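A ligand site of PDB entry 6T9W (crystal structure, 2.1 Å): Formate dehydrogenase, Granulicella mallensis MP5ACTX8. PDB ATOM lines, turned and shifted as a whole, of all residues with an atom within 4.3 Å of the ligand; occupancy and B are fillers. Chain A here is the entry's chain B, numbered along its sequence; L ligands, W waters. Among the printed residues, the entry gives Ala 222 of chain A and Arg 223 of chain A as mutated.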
ATOM      1  N   PHE A  99       8.642  28.295  10.948  1.00  0.00           N
ATOM      2  CA  PHE A  99       8.059  29.633  10.972  1.00  0.00           C
ATOM      3  C   PHE A  99       9.123  30.714  11.036  1.00  0.00           C
ATOM      4  O   PHE A  99       8.893  31.839  10.566  1.00  0.00           O
ATOM      5  CB  PHE A  99       7.110  29.739  12.171  1.00  0.00           C
ATOM      6  CG  PHE A  99       6.514  28.423  12.568  1.00  0.00           C
ATOM      7  CD1 PHE A  99       5.545  27.820  11.779  1.00  0.00           C
ATOM      8  CD2 PHE A  99       6.953  27.767  13.693  1.00  0.00           C
ATOM      9  CE1 PHE A  99       5.004  26.586  12.134  1.00  0.00           C
ATOM     10  CE2 PHE A  99       6.434  26.535  14.059  1.00  0.00           C
ATOM     11  CZ  PHE A  99       5.454  25.940  13.273  1.00  0.00           C
ATOM     12  N   ILE A 123       7.017  20.698  11.483  1.00  0.00           N
ATOM     13  CA  ILE A 123       6.942  19.726  10.403  1.00  0.00           C
ATOM     14  C   ILE A 123       7.499  20.347   9.125  1.00  0.00           C
ATOM     15  O   ILE A 123       7.170  21.498   8.804  1.00  0.00           O
ATOM     16  CB  ILE A 123       5.495  19.237  10.173  1.00  0.00           C
ATOM     17  CG1 ILE A 123       4.944  18.580  11.441  1.00  0.00           C
ATOM     18  CG2 ILE A 123       5.421  18.296   8.999  1.00  0.00           C
ATOM     19  CD1 ILE A 123       3.565  17.987  11.259  1.00  0.00           C
ATOM     20  N   GLY A 124       8.333  19.590   8.412  1.00  0.00           N
ATOM     21  CA  GLY A 124       8.881  20.055   7.148  1.00  0.00           C
ATOM     22  C   GLY A 124      10.307  20.550   7.274  1.00  0.00           C
ATOM     23  O   GLY A 124      10.548  21.624   7.847  1.00  0.00           O
ATOM     24  N   ASP A 126      12.630  21.074   4.741  1.00  0.00           N
ATOM     25  CA  ASP A 126      13.141  21.636   3.498  1.00  0.00           C
ATOM     26  C   ASP A 126      14.081  22.807   3.698  1.00  0.00           C
ATOM     27  O   ASP A 126      14.789  23.188   2.758  1.00  0.00           O
ATOM     28  CB  ASP A 126      11.960  22.097   2.659  1.00  0.00           C
ATOM     29  CG  ASP A 126      11.013  22.945   3.472  1.00  0.00           C
ATOM     30  OD1 ASP A 126      10.070  22.384   4.069  1.00  0.00           O
ATOM     31  OD2 ASP A 126      11.242  24.172   3.542  1.00  0.00           O
ATOM     32  N   ASN A 147       1.541  19.208  14.173  1.00  0.00           N
ATOM     33  CA  ASN A 147       0.638  20.310  13.874  1.00  0.00           C
ATOM     34  C   ASN A 147      -0.114  20.097  12.570  1.00  0.00           C
ATOM     35  O   ASN A 147      -0.637  21.067  12.005  1.00  0.00           O
ATOM     36  CB  ASN A 147       1.390  21.646  13.862  1.00  0.00           C
ATOM     37  CG  ASN A 147       2.512  21.684  12.833  1.00  0.00           C
ATOM     38  OD1 ASN A 147       2.569  20.863  11.921  1.00  0.00           O
ATOM     39  ND2 ASN A 147       3.409  22.656  12.973  1.00  0.00           N
ATOM     40  N   SER A 148      -0.183  18.857  12.078  1.00  0.00           N
ATOM     41  CA  SER A 148      -0.892  18.601  10.827  1.00  0.00           C
ATOM     42  C   SER A 148      -2.357  19.002  10.922  1.00  0.00           C
ATOM     43  O   SER A 148      -2.926  19.544   9.966  1.00  0.00           O
ATOM     44  CB  SER A 148      -0.778  17.123  10.457  1.00  0.00           C
ATOM     45  OG  SER A 148       0.577  16.739  10.306  1.00  0.00           O
ATOM     46  N   VAL A 151      -2.990  22.806  10.697  1.00  0.00           N
ATOM     47  CA  VAL A 151      -2.945  23.312   9.338  1.00  0.00           C
ATOM     48  C   VAL A 151      -4.255  23.023   8.615  1.00  0.00           C
ATOM     49  O   VAL A 151      -4.759  23.866   7.861  1.00  0.00           O
ATOM     50  CB  VAL A 151      -1.751  22.726   8.584  1.00  0.00           C
ATOM     51  CG1 VAL A 151      -1.749  23.157   7.137  1.00  0.00           C
ATOM     52  CG2 VAL A 151      -0.482  23.151   9.260  1.00  0.00           C
ATOM     53  N   VAL A 198      -3.641  18.636  -3.497  1.00  0.00           N
ATOM     54  CA  VAL A 198      -2.374  18.057  -3.907  1.00  0.00           C
ATOM     55  C   VAL A 198      -1.770  17.391  -2.674  1.00  0.00           C
ATOM     56  O   VAL A 198      -1.421  18.072  -1.710  1.00  0.00           O
ATOM     57  CB  VAL A 198      -1.434  19.106  -4.507  1.00  0.00           C
ATOM     58  CG1 VAL A 198      -0.079  18.482  -4.825  1.00  0.00           C
ATOM     59  CG2 VAL A 198      -2.043  19.709  -5.780  1.00  0.00           C
ATOM     60  N   ALA A 199      -1.689  16.060  -2.713  1.00  0.00           N
ATOM     61  CA  ALA A 199      -1.264  15.183  -1.613  1.00  0.00           C
ATOM     62  C   ALA A 199      -2.457  14.926  -0.695  1.00  0.00           C
ATOM     63  O   ALA A 199      -3.360  15.761  -0.591  1.00  0.00           O
ATOM     64  CB  ALA A 199      -0.025  15.720  -0.890  1.00  0.00           C
ATOM     65  N   GLY A 201      -1.672  13.293   2.575  1.00  0.00           N
ATOM     66  CA  GLY A 201      -0.990  12.808   3.767  1.00  0.00           C
ATOM     67  C   GLY A 201      -1.715  13.232   5.017  1.00  0.00           C
ATOM     68  O   GLY A 201      -2.946  13.324   5.041  1.00  0.00           O
ATOM     69  N   ARG A 202      -0.956  13.518   6.076  1.00  0.00           N
ATOM     70  CA  ARG A 202      -1.553  13.822   7.368  1.00  0.00           C
ATOM     71  C   ARG A 202      -2.404  15.082   7.296  1.00  0.00           C
ATOM     72  O   ARG A 202      -3.530  15.113   7.830  1.00  0.00           O
ATOM     73  CB  ARG A 202      -0.459  13.942   8.423  1.00  0.00           C
ATOM     74  CG  ARG A 202       0.122  12.582   8.792  1.00  0.00           C
ATOM     75  CD  ARG A 202       1.489  12.707   9.454  1.00  0.00           C
ATOM     76  NE  ARG A 202       2.024  11.390   9.800  1.00  0.00           N
ATOM     77  CZ  ARG A 202       2.829  10.676   9.022  1.00  0.00           C
ATOM     78  NH1 ARG A 202       3.214  11.140   7.844  1.00  0.00           N
ATOM     79  NH2 ARG A 202       3.273   9.491   9.436  1.00  0.00           N
ATOM     80  N   ILE A 203      -1.914  16.125   6.634  1.00  0.00           N
ATOM     81  CA  ILE A 203      -2.699  17.342   6.483  1.00  0.00           C
ATOM     82  C   ILE A 203      -3.814  17.132   5.448  1.00  0.00           C
ATOM     83  O   ILE A 203      -4.996  17.341   5.743  1.00  0.00           O
ATOM     84  CB  ILE A 203      -1.807  18.530   6.099  1.00  0.00           C
ATOM     85  CG1 ILE A 203      -0.878  18.896   7.259  1.00  0.00           C
ATOM     86  CG2 ILE A 203      -2.662  19.736   5.734  1.00  0.00           C
ATOM     87  CD1 ILE A 203       0.210  19.868   6.872  1.00  0.00           C
ATOM     88  N   PHE A 221      -4.895  14.400  -5.922  1.00  0.00           N
ATOM     89  CA  PHE A 221      -3.758  13.883  -6.649  1.00  0.00           C
ATOM     90  C   PHE A 221      -2.686  13.487  -5.639  1.00  0.00           C
ATOM     91  O   PHE A 221      -2.437  14.213  -4.671  1.00  0.00           O
ATOM     92  CB  PHE A 221      -3.189  14.916  -7.628  1.00  0.00           C
ATOM     93  CG  PHE A 221      -1.751  14.662  -8.006  1.00  0.00           C
ATOM     94  CD1 PHE A 221      -1.420  13.629  -8.872  1.00  0.00           C
ATOM     95  CD2 PHE A 221      -0.730  15.443  -7.497  1.00  0.00           C
ATOM     96  CE1 PHE A 221      -0.102  13.388  -9.223  1.00  0.00           C
ATOM     97  CE2 PHE A 221       0.593  15.207  -7.842  1.00  0.00           C
ATOM     98  CZ  PHE A 221       0.900  14.177  -8.705  1.00  0.00           C
ATOM     99  N   ALA A 222      -2.069  12.343  -5.884  1.00  0.00           N
ATOM    100  CA  ALA A 222      -0.944  11.892  -5.081  1.00  0.00           C
ATOM    101  C   ALA A 222      -0.157  10.891  -5.907  1.00  0.00           C
ATOM    102  O   ALA A 222      -0.668  10.316  -6.861  1.00  0.00           O
ATOM    103  CB  ALA A 222      -1.398  11.272  -3.755  1.00  0.00           C
ATOM    104  N   ARG A 223       1.107  10.703  -5.528  1.00  0.00           N
ATOM    105  CA  ARG A 223       1.925   9.700  -6.189  1.00  0.00           C
ATOM    106  C   ARG A 223       1.388   8.291  -5.961  1.00  0.00           C
ATOM    107  O   ARG A 223       1.672   7.395  -6.754  1.00  0.00           O
ATOM    108  CB  ARG A 223       3.371   9.821  -5.717  1.00  0.00           C
ATOM    109  CG  ARG A 223       4.085  11.041  -6.257  1.00  0.00           C
ATOM    110  CD  ARG A 223       5.431  11.223  -5.604  1.00  0.00           C
ATOM    111  NE  ARG A 223       5.353  11.057  -4.164  1.00  0.00           N
ATOM    112  CZ  ARG A 223       6.403  10.943  -3.362  1.00  0.00           C
ATOM    113  NH1 ARG A 223       7.634  10.992  -3.875  1.00  0.00           N
ATOM    114  NH2 ARG A 223       6.244  10.785  -2.053  1.00  0.00           N
ATOM    115  N   HIS A 224       0.583   8.091  -4.911  1.00  0.00           N
ATOM    116  CA  HIS A 224       0.008   6.793  -4.601  1.00  0.00           C
ATOM    117  C   HIS A 224      -1.402   6.975  -4.063  1.00  0.00           C
ATOM    118  O   HIS A 224      -1.707   7.962  -3.389  1.00  0.00           O
ATOM    119  CB  HIS A 224       0.880   6.027  -3.596  1.00  0.00           C
ATOM    120  CG  HIS A 224       2.304   5.856  -4.037  1.00  0.00           C
ATOM    121  ND1 HIS A 224       3.341   6.544  -3.462  1.00  0.00           N
ATOM    122  CD2 HIS A 224       2.841   5.115  -5.035  1.00  0.00           C
ATOM    123  CE1 HIS A 224       4.470   6.212  -4.065  1.00  0.00           C
ATOM    124  NE2 HIS A 224       4.193   5.342  -5.027  1.00  0.00           N
ATOM    125  N   ASN A 255      -0.840  20.461  -0.228  1.00  0.00           N
ATOM    126  CA  ASN A 255      -0.481  19.893   1.072  1.00  0.00           C
ATOM    127  C   ASN A 255       0.669  18.888   0.949  1.00  0.00           C
ATOM    128  O   ASN A 255       0.734  17.922   1.728  1.00  0.00           O
ATOM    129  CB  ASN A 255      -1.701  19.238   1.737  1.00  0.00           C
ATOM    130  CG  ASN A 255      -2.855  20.207   1.917  1.00  0.00           C
ATOM    131  OD1 ASN A 255      -3.867  20.127   1.220  1.00  0.00           O
ATOM    132  ND2 ASN A 255      -2.689  21.158   2.838  1.00  0.00           N
ATOM    133  N   ALA A 256       1.565  19.093  -0.003  1.00  0.00           N
ATOM    134  CA  ALA A 256       2.716  18.239  -0.232  1.00  0.00           C
ATOM    135  C   ALA A 256       3.974  18.887   0.327  1.00  0.00           C
ATOM    136  O   ALA A 256       4.031  20.121   0.455  1.00  0.00           O
ATOM    137  CB  ALA A 256       2.904  17.983  -1.742  1.00  0.00           C
ATOM    138  N   PRO A 257       5.002  18.107   0.666  1.00  0.00           N
ATOM    139  CA  PRO A 257       6.258  18.713   1.125  1.00  0.00           C
ATOM    140  C   PRO A 257       6.976  19.414  -0.016  1.00  0.00           C
ATOM    141  O   PRO A 257       6.685  19.203  -1.192  1.00  0.00           O
ATOM    142  CB  PRO A 257       7.073  17.516   1.631  1.00  0.00           C
ATOM    143  CG  PRO A 257       6.133  16.339   1.639  1.00  0.00           C
ATOM    144  CD  PRO A 257       5.098  16.638   0.608  1.00  0.00           C
ATOM    145  N   HIS A 259      10.111  19.479  -2.102  1.00  0.00           N
ATOM    146  CA  HIS A 259      11.233  18.661  -2.523  1.00  0.00           C
ATOM    147  C   HIS A 259      11.297  18.718  -4.049  1.00  0.00           C
ATOM    148  O   HIS A 259      10.429  19.365  -4.655  1.00  0.00           O
ATOM    149  CB  HIS A 259      11.115  17.242  -1.937  1.00  0.00           C
ATOM    150  CG  HIS A 259      10.036  16.408  -2.552  1.00  0.00           C
ATOM    151  ND1 HIS A 259      10.182  15.787  -3.775  1.00  0.00           N
ATOM    152  CD2 HIS A 259       8.828  16.023  -2.071  1.00  0.00           C
ATOM    153  CE1 HIS A 259       9.088  15.092  -4.039  1.00  0.00           C
ATOM    154  NE2 HIS A 259       8.261  15.214  -3.020  1.00  0.00           N
ATOM    155  N   GLY A 261      10.311  17.052  -6.468  1.00  0.00           N
ATOM    156  CA  GLY A 261       9.086  16.717  -7.183  1.00  0.00           C
ATOM    157  C   GLY A 261       7.996  17.769  -7.080  1.00  0.00           C
ATOM    158  O   GLY A 261       7.031  17.712  -7.846  1.00  0.00           O
ATOM    159  N   THR A 262       8.109  18.717  -6.145  1.00  0.00           N
ATOM    160  CA  THR A 262       7.083  19.724  -5.932  1.00  0.00           C
ATOM    161  C   THR A 262       7.572  21.150  -6.075  1.00  0.00           C
ATOM    162  O   THR A 262       6.742  22.067  -6.085  1.00  0.00           O
ATOM    163  CB  THR A 262       6.460  19.563  -4.529  1.00  0.00           C
ATOM    164  OG1 THR A 262       7.470  19.732  -3.529  1.00  0.00           O
ATOM    165  CG2 THR A 262       5.810  18.201  -4.392  1.00  0.00           C
ATOM    166  N   THR A 283      -0.875  26.179   2.244  1.00  0.00           N
ATOM    167  CA  THR A 283      -0.274  26.131   3.573  1.00  0.00           C
ATOM    168  C   THR A 283       0.856  25.115   3.632  1.00  0.00           C
ATOM    169  O   THR A 283       1.191  24.638   4.730  1.00  0.00           O
ATOM    170  CB  THR A 283      -1.316  25.739   4.610  1.00  0.00           C
ATOM    171  OG1 THR A 283      -1.842  24.447   4.283  1.00  0.00           O
ATOM    172  CG2 THR A 283      -2.445  26.761   4.648  1.00  0.00           C
ATOM    173  N   ALA A 284       1.432  24.750   2.488  1.00  0.00           N
ATOM    174  CA  ALA A 284       2.510  23.761   2.467  1.00  0.00           C
ATOM    175  C   ALA A 284       3.912  24.349   2.534  1.00  0.00           C
ATOM    176  O   ALA A 284       4.572  24.260   3.569  1.00  0.00           O
ATOM    177  CB  ALA A 284       2.416  22.903   1.208  1.00  0.00           C
ATOM    178  N   ARG A 285       4.371  24.929   1.435  1.00  0.00           N
ATOM    179  CA  ARG A 285       5.595  25.737   1.416  1.00  0.00           C
ATOM    180  C   ARG A 285       5.469  26.727   0.276  1.00  0.00           C
ATOM    181  O   ARG A 285       4.910  26.413  -0.776  1.00  0.00           O
ATOM    182  CB  ARG A 285       6.857  24.879   1.247  1.00  0.00           C
ATOM    183  CG  ARG A 285       7.250  24.070   2.485  1.00  0.00           C
ATOM    184  CD  ARG A 285       7.592  24.964   3.669  1.00  0.00           C
ATOM    185  NE  ARG A 285       8.202  24.238   4.780  1.00  0.00           N
ATOM    186  CZ  ARG A 285       7.595  23.944   5.928  1.00  0.00           C
ATOM    187  NH1 ARG A 285       6.333  24.315   6.130  1.00  0.00           N
ATOM    188  NH2 ARG A 285       8.228  23.275   6.879  1.00  0.00           N
ATOM    189  N   ASP A 309      -0.242  30.619   4.321  1.00  0.00           N
ATOM    190  CA  ASP A 309       0.570  31.207   5.376  1.00  0.00           C
ATOM    191  C   ASP A 309       2.067  31.060   5.123  1.00  0.00           C
ATOM    192  O   ASP A 309       2.848  31.558   5.930  1.00  0.00           O
ATOM    193  CB  ASP A 309       0.194  30.616   6.736  1.00  0.00           C
ATOM    194  CG  ASP A 309       0.442  29.128   6.833  1.00  0.00           C
ATOM    195  OD1 ASP A 309       0.392  28.444   5.795  1.00  0.00           O
ATOM    196  OD2 ASP A 309       0.711  28.640   7.961  1.00  0.00           O
ATOM    197  N   VAL A 310       2.484  30.429   4.026  1.00  0.00           N
ATOM    198  CA  VAL A 310       3.890  30.118   3.814  1.00  0.00           C
ATOM    199  C   VAL A 310       4.439  30.928   2.643  1.00  0.00           C
ATOM    200  O   VAL A 310       3.737  31.165   1.640  1.00  0.00           O
ATOM    201  CB  VAL A 310       4.099  28.610   3.592  1.00  0.00           C
ATOM    202  CG1 VAL A 310       3.918  27.870   4.917  1.00  0.00           C
ATOM    203  CG2 VAL A 310       3.125  28.092   2.545  1.00  0.00           C
ATOM    204  N   HIS A 333       3.595  32.941   8.618  1.00  0.00           N
ATOM    205  CA  HIS A 333       3.668  31.487   8.786  1.00  0.00           C
ATOM    206  C   HIS A 333       3.291  31.130  10.217  1.00  0.00           C
ATOM    207  O   HIS A 333       4.152  30.988  11.086  1.00  0.00           O
ATOM    208  CB  HIS A 333       5.056  30.980   8.418  1.00  0.00           C
ATOM    209  CG  HIS A 333       5.152  29.489   8.391  1.00  0.00           C
ATOM    210  ND1 HIS A 333       6.333  28.815   8.158  1.00  0.00           N
ATOM    211  CD2 HIS A 333       4.199  28.528   8.548  1.00  0.00           C
ATOM    212  CE1 HIS A 333       6.105  27.513   8.183  1.00  0.00           C
ATOM    213  NE2 HIS A 333       4.824  27.310   8.421  1.00  0.00           N
ATOM    214  N   SER A 335       0.163  28.899  11.015  1.00  0.00           N
ATOM    215  CA  SER A 335      -0.840  27.861  11.251  1.00  0.00           C
ATOM    216  C   SER A 335      -0.260  26.727  12.088  1.00  0.00           C
ATOM    217  O   SER A 335      -0.936  26.203  12.985  1.00  0.00           O
ATOM    218  CB  SER A 335      -1.394  27.324   9.928  1.00  0.00           C
ATOM    219  OG  SER A 335      -0.478  26.482   9.266  1.00  0.00           O
ATOM    220  N   GLY A 336       0.986  26.342  11.835  1.00  0.00           N
ATOM    221  CA  GLY A 336       1.635  25.313  12.618  1.00  0.00           C
ATOM    222  C   GLY A 336       2.198  25.743  13.949  1.00  0.00           C
ATOM    223  O   GLY A 336       2.758  24.915  14.662  1.00  0.00           O
ATOM    224  N   THR A 377      10.151   8.849   7.626  1.00  0.00           N
ATOM    225  CA  THR A 377       9.193   9.634   6.851  1.00  0.00           C
ATOM    226  C   THR A 377       9.846  10.313   5.661  1.00  0.00           C
ATOM    227  O   THR A 377       9.215  10.467   4.616  1.00  0.00           O
ATOM    228  CB  THR A 377       8.508  10.658   7.755  1.00  0.00           C
ATOM    229  OG1 THR A 377       7.867  10.000   8.849  1.00  0.00           O
ATOM    230  CG2 THR A 377       7.477  11.458   6.969  1.00  0.00           C
ATOM    231  N   HIS A 380       9.559   8.337   2.790  1.00  0.00           N
ATOM    232  CA  HIS A 380       8.191   8.192   2.302  1.00  0.00           C
ATOM    233  C   HIS A 380       7.694   9.434   1.571  1.00  0.00           C
ATOM    234  O   HIS A 380       6.922   9.310   0.613  1.00  0.00           O
ATOM    235  CB  HIS A 380       7.239   7.867   3.453  1.00  0.00           C
ATOM    236  CG  HIS A 380       7.555   6.587   4.166  1.00  0.00           C
ATOM    237  ND1 HIS A 380       7.665   6.508   5.541  1.00  0.00           N
ATOM    238  CD2 HIS A 380       7.776   5.336   3.698  1.00  0.00           C
ATOM    239  CE1 HIS A 380       7.938   5.266   5.883  1.00  0.00           C
ATOM    240  NE2 HIS A 380       8.013   4.537   4.791  1.00  0.00           N
ATOM    241  N   SER A 381       8.099  10.633   2.001  1.00  0.00           N
ATOM    242  CA  SER A 381       7.459  11.859   1.553  1.00  0.00           C
ATOM    243  C   SER A 381       8.336  12.767   0.695  1.00  0.00           C
ATOM    244  O   SER A 381       7.807  13.505  -0.125  1.00  0.00           O
ATOM    245  CB  SER A 381       6.949  12.662   2.763  1.00  0.00           C
ATOM    246  OG  SER A 381       5.890  11.982   3.419  1.00  0.00           O
ATOM    247  N   TYR A 382       9.651  12.727   0.888  1.00  0.00           N
ATOM    248  CA  TYR A 382      10.549  13.583   0.135  1.00  0.00           C
ATOM    249  C   TYR A 382      11.306  12.792  -0.929  1.00  0.00           C
ATOM    250  O   TYR A 382      11.168  11.567  -1.044  1.00  0.00           O
ATOM    251  CB  TYR A 382      11.564  14.271   1.062  1.00  0.00           C
ATOM    252  CG  TYR A 382      10.976  15.221   2.086  1.00  0.00           C
ATOM    253  CD1 TYR A 382      10.187  14.762   3.130  1.00  0.00           C
ATOM    254  CD2 TYR A 382      11.243  16.586   2.016  1.00  0.00           C
ATOM    255  CE1 TYR A 382       9.674  15.624   4.068  1.00  0.00           C
ATOM    256  CE2 TYR A 382      10.724  17.466   2.947  1.00  0.00           C
ATOM    257  CZ  TYR A 382       9.945  16.980   3.972  1.00  0.00           C
ATOM    258  OH  TYR A 382       9.424  17.846   4.900  1.00  0.00           O
HETATM  259  P1  LIG L   1       2.958  13.996   5.396  1.00  0.00           P
HETATM  260  O1  LIG L   1       4.289  13.313   5.094  1.00  0.00           O
HETATM  261  O2  LIG L   1       2.106  13.207   6.384  1.00  0.00           O
HETATM  262  O3  LIG L   1       2.099  14.153   4.006  1.00  0.00           O
HETATM  263  C1  LIG L   1       2.861  14.512   2.908  1.00  0.00           C
HETATM  264  C2  LIG L   1       2.248  13.759   1.695  1.00  0.00           C
HETATM  265  O4  LIG L   1       2.792  14.492   0.452  1.00  0.00           O
HETATM  266  C3  LIG L   1       2.684  12.575   1.621  1.00  0.00           C
HETATM  267  O5  LIG L   1       1.610  11.644   2.013  1.00  0.00           O
HETATM  268  C4  LIG L   1       3.094  12.300   0.037  1.00  0.00           C
HETATM  269  O6  LIG L   1       2.245  11.178  -0.400  1.00  0.00           O
HETATM  270  C5  LIG L   1       2.692  13.355  -0.537  1.00  0.00           C
HETATM  271  N1  LIG L   1       3.370  13.820  -1.831  1.00  0.00           N
HETATM  272  C6  LIG L   1       4.683  13.695  -1.563  1.00  0.00           C
HETATM  273  N2  LIG L   1       5.326  14.111  -2.694  1.00  0.00           N
HETATM  274  C7  LIG L   1       4.396  14.483  -3.610  1.00  0.00           C
HETATM  275  C8  LIG L   1       4.423  14.967  -4.896  1.00  0.00           C
HETATM  276  N3  LIG L   1       5.747  15.162  -5.526  1.00  0.00           N
HETATM  277  N4  LIG L   1       3.281  15.241  -5.534  1.00  0.00           N
HETATM  278  C9  LIG L   1       2.058  15.041  -4.922  1.00  0.00           C
HETATM  279  N5  LIG L   1       2.024  14.560  -3.676  1.00  0.00           N
HETATM  280  C10 LIG L   1       3.186  14.292  -3.044  1.00  0.00           C
HETATM  281  O7  LIG L   1       3.257  15.511   6.023  1.00  0.00           O
HETATM  282  P2  LIG L   1       2.029  16.592   6.402  1.00  0.00           P
HETATM  283  O8  LIG L   1       0.780  16.265   5.643  1.00  0.00           O
HETATM  284  O9  LIG L   1       1.782  16.528   7.876  1.00  0.00           O
HETATM  285  O10 LIG L   1       2.605  18.067   5.939  1.00  0.00           O
HETATM  286  C11 LIG L   1       2.980  18.165   4.545  1.00  0.00           C
HETATM  287  C12 LIG L   1       3.801  19.380   4.345  1.00  0.00           C
HETATM  288  O11 LIG L   1       2.943  20.674   4.806  1.00  0.00           O
HETATM  289  C13 LIG L   1       4.860  19.365   5.129  1.00  0.00           C
HETATM  290  O12 LIG L   1       6.019  18.680   4.471  1.00  0.00           O
HETATM  291  C14 LIG L   1       5.171  20.821   5.324  1.00  0.00           C
HETATM  292  O13 LIG L   1       6.001  21.269   4.329  1.00  0.00           O
HETATM  293  C15 LIG L   1       3.777  21.540   5.215  1.00  0.00           C
HETATM  294  N6  LIG L   1       3.401  22.028   6.595  1.00  0.00           N
HETATM  295  C16 LIG L   1       3.072  23.316   6.773  1.00  0.00           C
HETATM  296  C17 LIG L   1       2.728  23.773   8.049  1.00  0.00           C
HETATM  297  C18 LIG L   1       2.337  25.220   8.282  1.00  0.00           C
HETATM  298  O14 LIG L   1       1.791  25.867   7.422  1.00  0.00           O
HETATM  299  N7  LIG L   1       2.611  25.804   9.547  1.00  0.00           N
HETATM  300  C19 LIG L   1       2.754  22.916   9.102  1.00  0.00           C
HETATM  301  C20 LIG L   1       3.083  21.606   8.924  1.00  0.00           C
HETATM  302  C21 LIG L   1       3.422  21.162   7.658  1.00  0.00           C
HETATM  303  P3  LIG L   1       2.599  10.348  -1.787  1.00  0.00           P
HETATM  304  O15 LIG L   1       1.462   9.432  -2.110  1.00  0.00           O
HETATM  305  O16 LIG L   1       2.831  11.294  -2.932  1.00  0.00           O
HETATM  306  O17 LIG L   1       3.845   9.523  -1.531  1.00  0.00           O
HETATM  307  O   HOH W   1       7.433  17.198   6.313  1.00  0.00           O
HETATM  308  O   HOH W   2       8.697  20.405   3.306  1.00  0.00           O
HETATM  309  O   HOH W   3       3.618  15.146   9.591  1.00  0.00           O
HETATM  310  O   HOH W   4       0.527   7.972  -0.213  1.00  0.00           O
HETATM  311  O   HOH W   5       1.446  10.975   4.856  1.00  0.00           O
HETATM  312  O   HOH W   6       3.840   8.368   1.017  1.00  0.00           O
HETATM  313  O   HOH W   7      -0.715  16.130   3.376  1.00  0.00           O
HETATM  314  O   HOH W   8      -0.833  11.616  -0.246  1.00  0.00           O
HETATM  315  O   HOH W   9       6.663  14.407   6.348  1.00  0.00           O
HETATM  316  O   HOH W  10       8.306  13.257  -6.689  1.00  0.00           O
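Water W7 lies within hydrogen-bond range of O8 of the ligand (2.7 Å), O of Asn 255 (2.8 Å), N of Gly 201 (3.1 Å) and N of Ile 203 (3.5 Å). Water W1 lies within hydrogen-bond range of OH of Tyr 382, O12 of the ligand and N of Gly 124. Water W5 lies within hydrogen-bond range of O2 of the ligand (2.8 Å) and NH1 of Arg 202 (3.5 Å). Water W6 bridges O17 of the ligand (2.8 Å) and O of His 380 (3.2 Å). Water W2 lies within hydrogen-bond range of OD1 of Asp 126 (2.5 Å), O13 of the ligand (3.0 Å) and OH of Tyr 382 (3.1 Å). Water W8 bridges an oxygen (O6) of the ligand (3.1 Å) and the backbone NH of Gly 201 (3.4 Å).
A ring nitrogen (ND1) of His 259 is in hydrogen-bond range of the backbone NH of Gly 261, at 3.0 Å. NH2 of Arg 285 is in hydrogen-bond range of O of Gly 124 (3.0 Å). The side-chain carboxylate (OD1) of Asp 126 is in salt-bridge range of the guanidinium group (NE) of Arg 285, at 2.7 Å. The backbone carbonyl oxygen (O) of Gly 336 sits at hydrogen-bond distance from the side-chain amide nitrogen (ND2) of Asn 147 (2.9 Å). The backbone NH of Ala 199 sits at hydrogen-bond distance from the backbone carbonyl oxygen of Phe 221. OD2 of Asp 309 lies within hydrogen-bond range of OG of Ser 335. The backbone NH (N) of Asn 255 is in hydrogen-bond range of the backbone carbonyl oxygen (O) of Val 198, at 2.9 Å. O of Asp 309 sits close to N of His 333.
O14 of the ligand sits close to O of Thr 283 (3.0 Å). OD2 of Asp 309 sits close to O14 of the ligand (3.0 Å). N7 of the ligand sits close to N of Gly 336 (2.9 Å). Residues that only touch the ligand: Asn 147 (3.1 Å), Pro 257 (3.2 Å), Thr 262 (3.2 Å), Val 151 (3.2 Å), Phe 221 (3.3 Å), Gly 201 (3.3 Å), Ala 199 (3.4 Å), Arg 285 (3.5 Å), Tyr 382 (3.5 Å), Ile 123 (3.6 Å), Phe 99 (3.6 Å), Asn 255 (3.6 Å), Gly 261 (3.7 Å), His 380 (3.8 Å), Ala 222 (3.8 Å), Ala 256 (3.8 Å) and Val 310 (3.8 Å). Hydrophobic or aromatic side chains within 4 Å of the ligand: Phe 99, Ile 123, Val 151, Ala 199, Ile 203, Phe 221, Ala 222, His 224, Ala 256, Pro 257, His 259, Val 310 and His 333. 30 residues have an atom within 4 Å of the ligand: Phe 99, Ile 123, Asn 147, Ser 148, Val 151, Ala 199, Gly 201, Arg 202, Ile 203, Phe 221, Ala 222, Arg 223, His 224, Asn 255, Ala 256, Pro 257, His 259, Gly 261, Thr 262, Thr 283, Ala 284, Arg 285, Asp 309, Val 310, His 333, Ser 335, Gly 336, His 380, Ser 381 and Tyr 382.
An oxygen (O1) of the ligand is in hydrogen-bond range of the side-chain hydroxyl (OG) of Ser 381 (2.7 Å). The guanidinium group (NH2) of Arg 223 lies within salt-bridge range of an oxygen (O17) of the ligand (2.8 Å). An oxygen (O15) of the ligand is in hydrogen-bond range of the backbone NH of His 224 (3.2 Å). O9 of the ligand lies within hydrogen-bond range of OG of Ser 148 (2.7 Å). The guanidinium group of Arg 202 is in salt-bridge range of an oxygen (O2) of the ligand. An oxygen (O2) of the ligand lies within hydrogen-bond range of the backbone NH (N) of Arg 202 (3.1 Å). A ring nitrogen (NE2) of His 333 lies within hydrogen-bond range of a nitrogen (N7) of the ligand, at 2.9 Å. A ring nitrogen (NE2) of His 259 sits at hydrogen-bond distance from a nitrogen (N2) of the ligand (3.2 Å). O14 of the ligand lies within hydrogen-bond range of OG of Ser 335, 3.0 Å away. The backbone carbonyl oxygen of Ala 284 lies close to an oxygen (O13) of the ligand (3.4 Å). An oxygen (O8) of the ligand lies within hydrogen-bond range of the backbone NH of Ile 203 (2.9 Å). The backbone NH (N) of Arg 223 sits at hydrogen-bond distance from an oxygen (O16) of the ligand (3.2 Å).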
